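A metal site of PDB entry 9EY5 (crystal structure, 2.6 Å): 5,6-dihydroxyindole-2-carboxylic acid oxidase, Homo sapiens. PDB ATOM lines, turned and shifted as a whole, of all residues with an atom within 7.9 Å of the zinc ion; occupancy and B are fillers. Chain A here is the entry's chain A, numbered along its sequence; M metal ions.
Of the 14 residues printed, 3 come within 4 Å of the zinc ion.
The zinc ion is bound by the side-chain carboxylate (OE2) of Glu 64 (2.1 Å), a ring nitrogen (NE2) of His 57 (2.2 Å) and a ring nitrogen (NE2) of His 51 (2.2 Å). Slightly farther from the zinc ion lies OE1 of Glu 64 (2.8 Å).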
ATOM      1  N   ARG A  49      27.029 -16.873  27.610  1.00  0.00           N
ATOM      2  CA  ARG A  49      28.179 -17.532  28.192  1.00  0.00           C
ATOM      3  C   ARG A  49      28.826 -18.432  27.135  1.00  0.00           C
ATOM      4  O   ARG A  49      28.177 -18.841  26.164  1.00  0.00           O
ATOM      5  CB  ARG A  49      27.759 -18.349  29.434  1.00  0.00           C
ATOM      6  CG  ARG A  49      27.823 -17.600  30.797  1.00  0.00           C
ATOM      7  CD  ARG A  49      26.384 -17.348  31.286  1.00  0.00           C
ATOM      8  NE  ARG A  49      26.163 -16.754  32.599  1.00  0.00           N
ATOM      9  CZ  ARG A  49      25.806 -15.483  32.762  1.00  0.00           C
ATOM     10  NH1 ARG A  49      25.671 -14.666  31.742  1.00  0.00           N
ATOM     11  NH2 ARG A  49      25.568 -15.024  34.007  1.00  0.00           N
ATOM     12  N   PRO A  50      30.112 -18.702  27.264  1.00  0.00           N
ATOM     13  CA  PRO A  50      30.837 -19.428  26.190  1.00  0.00           C
ATOM     14  C   PRO A  50      30.555 -20.927  26.154  1.00  0.00           C
ATOM     15  O   PRO A  50      30.173 -21.533  27.158  1.00  0.00           O
ATOM     16  CB  PRO A  50      32.333 -19.145  26.495  1.00  0.00           C
ATOM     17  CG  PRO A  50      32.341 -18.939  27.969  1.00  0.00           C
ATOM     18  CD  PRO A  50      31.024 -18.315  28.380  1.00  0.00           C
ATOM     19  N   HIS A  51      30.703 -21.496  24.977  1.00  0.00           N
ATOM     20  CA  HIS A  51      30.490 -22.921  24.783  1.00  0.00           C
ATOM     21  C   HIS A  51      31.816 -23.638  24.526  1.00  0.00           C
ATOM     22  O   HIS A  51      32.867 -23.007  24.356  1.00  0.00           O
ATOM     23  CB  HIS A  51      29.509 -23.167  23.638  1.00  0.00           C
ATOM     24  CG  HIS A  51      29.936 -22.509  22.359  1.00  0.00           C
ATOM     25  ND1 HIS A  51      31.015 -22.945  21.609  1.00  0.00           N
ATOM     26  CD2 HIS A  51      29.407 -21.462  21.677  1.00  0.00           C
ATOM     27  CE1 HIS A  51      31.133 -22.191  20.535  1.00  0.00           C
ATOM     28  NE2 HIS A  51      30.174 -21.285  20.554  1.00  0.00           N
ATOM     29  N   SER A  52      31.745 -24.964  24.509  1.00  0.00           N
ATOM     30  CA  SER A  52      32.918 -25.774  24.277  1.00  0.00           C
ATOM     31  C   SER A  52      33.460 -25.512  22.871  1.00  0.00           C
ATOM     32  O   SER A  52      32.713 -25.123  21.961  1.00  0.00           O
ATOM     33  CB  SER A  52      32.588 -27.249  24.434  1.00  0.00           C
ATOM     34  OG  SER A  52      31.533 -27.597  23.571  1.00  0.00           O
ATOM     35  N   GLN A  54      34.953 -25.642  19.024  1.00  0.00           N
ATOM     36  CA  GLN A  54      34.741 -26.352  17.774  1.00  0.00           C
ATOM     37  C   GLN A  54      35.778 -25.881  16.763  1.00  0.00           C
ATOM     38  O   GLN A  54      35.975 -24.674  16.607  1.00  0.00           O
ATOM     39  CB  GLN A  54      33.353 -26.103  17.185  1.00  0.00           C
ATOM     40  CG  GLN A  54      32.209 -26.219  18.157  1.00  0.00           C
ATOM     41  CD  GLN A  54      31.050 -25.331  17.736  1.00  0.00           C
ATOM     42  OE1 GLN A  54      31.077 -24.703  16.675  1.00  0.00           O
ATOM     43  NE2 GLN A  54      30.022 -25.261  18.590  1.00  0.00           N
ATOM     44  N   HIS A  57      34.984 -23.115  13.450  1.00  0.00           N
ATOM     45  CA  HIS A  57      33.722 -22.570  13.962  1.00  0.00           C
ATOM     46  C   HIS A  57      33.666 -21.089  13.578  1.00  0.00           C
ATOM     47  O   HIS A  57      34.298 -20.241  14.228  1.00  0.00           O
ATOM     48  CB  HIS A  57      33.611 -22.770  15.471  1.00  0.00           C
ATOM     49  CG  HIS A  57      32.767 -21.737  16.141  1.00  0.00           C
ATOM     50  ND1 HIS A  57      33.301 -20.646  16.780  1.00  0.00           N
ATOM     51  CD2 HIS A  57      31.430 -21.623  16.237  1.00  0.00           C
ATOM     52  CE1 HIS A  57      32.318 -19.897  17.256  1.00  0.00           C
ATOM     53  NE2 HIS A  57      31.174 -20.453  16.916  1.00  0.00           N
ATOM     54  N   ASP A  58      32.898 -20.795  12.532  1.00  0.00           N
ATOM     55  CA  ASP A  58      32.786 -19.417  12.066  1.00  0.00           C
ATOM     56  C   ASP A  58      31.925 -18.572  13.010  1.00  0.00           C
ATOM     57  O   ASP A  58      32.205 -17.379  13.202  1.00  0.00           O
ATOM     58  CB  ASP A  58      32.224 -19.382  10.642  1.00  0.00           C
ATOM     59  CG  ASP A  58      30.853 -20.061  10.513  1.00  0.00           C
ATOM     60  OD1 ASP A  58      30.276 -20.469  11.543  1.00  0.00           O
ATOM     61  OD2 ASP A  58      30.350 -20.191   9.372  1.00  0.00           O
ATOM     62  N   GLY A  59      30.906 -19.177  13.613  1.00  0.00           N
ATOM     63  CA  GLY A  59      29.970 -18.418  14.418  1.00  0.00           C
ATOM     64  C   GLY A  59      28.895 -17.690  13.627  1.00  0.00           C
ATOM     65  O   GLY A  59      28.241 -16.804  14.186  1.00  0.00           O
ATOM     66  N   ARG A  60      28.729 -18.035  12.348  1.00  0.00           N
ATOM     67  CA  ARG A  60      27.694 -17.490  11.480  1.00  0.00           C
ATOM     68  C   ARG A  60      26.393 -18.251  11.601  1.00  0.00           C
ATOM     69  O   ARG A  60      25.419 -17.915  10.908  1.00  0.00           O
ATOM     70  CB  ARG A  60      28.166 -17.516  10.024  1.00  0.00           C
ATOM     71  CG  ARG A  60      29.513 -16.811   9.820  1.00  0.00           C
ATOM     72  CD  ARG A  60      29.436 -15.397  10.424  1.00  0.00           C
ATOM     73  NE  ARG A  60      28.249 -14.686   9.956  1.00  0.00           N
ATOM     74  CZ  ARG A  60      28.284 -13.558   9.262  1.00  0.00           C
ATOM     75  NH1 ARG A  60      29.423 -12.927   9.040  1.00  0.00           N
ATOM     76  NH2 ARG A  60      27.149 -13.035   8.808  1.00  0.00           N
ATOM     77  N   ASP A  61      26.360 -19.264  12.468  1.00  0.00           N
ATOM     78  CA  ASP A  61      25.215 -20.159  12.557  1.00  0.00           C
ATOM     79  C   ASP A  61      24.016 -19.435  13.171  1.00  0.00           C
ATOM     80  O   ASP A  61      24.088 -18.968  14.319  1.00  0.00           O
ATOM     81  CB  ASP A  61      25.591 -21.387  13.386  1.00  0.00           C
ATOM     82  CG  ASP A  61      24.492 -22.450  13.395  1.00  0.00           C
ATOM     83  OD1 ASP A  61      23.301 -22.085  13.503  1.00  0.00           O
ATOM     84  OD2 ASP A  61      24.824 -23.658  13.295  1.00  0.00           O
ATOM     85  N   GLU A  64      23.229 -19.688  17.001  1.00  0.00           N
ATOM     86  CA  GLU A  64      23.952 -19.026  18.083  1.00  0.00           C
ATOM     87  C   GLU A  64      23.055 -17.980  18.741  1.00  0.00           C
ATOM     88  O   GLU A  64      22.283 -17.294  18.070  1.00  0.00           O
ATOM     89  CB  GLU A  64      25.228 -18.357  17.560  1.00  0.00           C
ATOM     90  CG  GLU A  64      26.246 -19.297  16.957  1.00  0.00           C
ATOM     91  CD  GLU A  64      27.458 -19.512  17.846  1.00  0.00           C
ATOM     92  OE1 GLU A  64      27.326 -19.433  19.091  1.00  0.00           O
ATOM     93  OE2 GLU A  64      28.537 -19.761  17.290  1.00  0.00           O
ATOM     94  N   VAL A  65      23.198 -17.864  20.061  1.00  0.00           N
ATOM     95  CA  VAL A  65      22.442 -16.943  20.903  1.00  0.00           C
ATOM     96  C   VAL A  65      20.995 -16.827  20.437  1.00  0.00           C
ATOM     97  O   VAL A  65      20.459 -15.720  20.269  1.00  0.00           O
ATOM     98  CB  VAL A  65      23.137 -15.563  21.005  1.00  0.00           C
ATOM     99  CG1 VAL A  65      24.419 -15.725  21.770  1.00  0.00           C
ATOM    100  CG2 VAL A  65      23.416 -14.942  19.643  1.00  0.00           C
ATOM    101  N   ILE A 408      27.574 -26.291  22.228  1.00  0.00           N
ATOM    102  CA  ILE A 408      26.681 -25.186  21.883  1.00  0.00           C
ATOM    103  C   ILE A 408      25.235 -25.686  21.877  1.00  0.00           C
ATOM    104  O   ILE A 408      24.929 -26.797  21.421  1.00  0.00           O
ATOM    105  CB  ILE A 408      27.066 -24.541  20.540  1.00  0.00           C
ATOM    106  CG1 ILE A 408      26.235 -23.259  20.321  1.00  0.00           C
ATOM    107  CG2 ILE A 408      26.883 -25.497  19.387  1.00  0.00           C
ATOM    108  CD1 ILE A 408      26.389 -22.631  18.936  1.00  0.00           C
ATOM    109  N   TYR A 414      20.793 -21.290  27.992  1.00  0.00           N
ATOM    110  CA  TYR A 414      20.485 -21.222  26.560  1.00  0.00           C
ATOM    111  C   TYR A 414      18.980 -21.278  26.320  1.00  0.00           C
ATOM    112  O   TYR A 414      18.261 -22.042  26.973  1.00  0.00           O
ATOM    113  CB  TYR A 414      21.165 -22.391  25.819  1.00  0.00           C
ATOM    114  CG  TYR A 414      21.766 -22.001  24.497  1.00  0.00           C
ATOM    115  CD1 TYR A 414      20.995 -21.953  23.351  1.00  0.00           C
ATOM    116  CD2 TYR A 414      23.113 -21.668  24.398  1.00  0.00           C
ATOM    117  CE1 TYR A 414      21.537 -21.574  22.131  1.00  0.00           C
ATOM    118  CE2 TYR A 414      23.676 -21.294  23.197  1.00  0.00           C
ATOM    119  CZ  TYR A 414      22.892 -21.245  22.064  1.00  0.00           C
ATOM    120  OH  TYR A 414      23.451 -20.858  20.860  1.00  0.00           O
HETATM  121 ZN    ZN M   1      30.010 -20.001  18.742  1.00  0.00          ZN
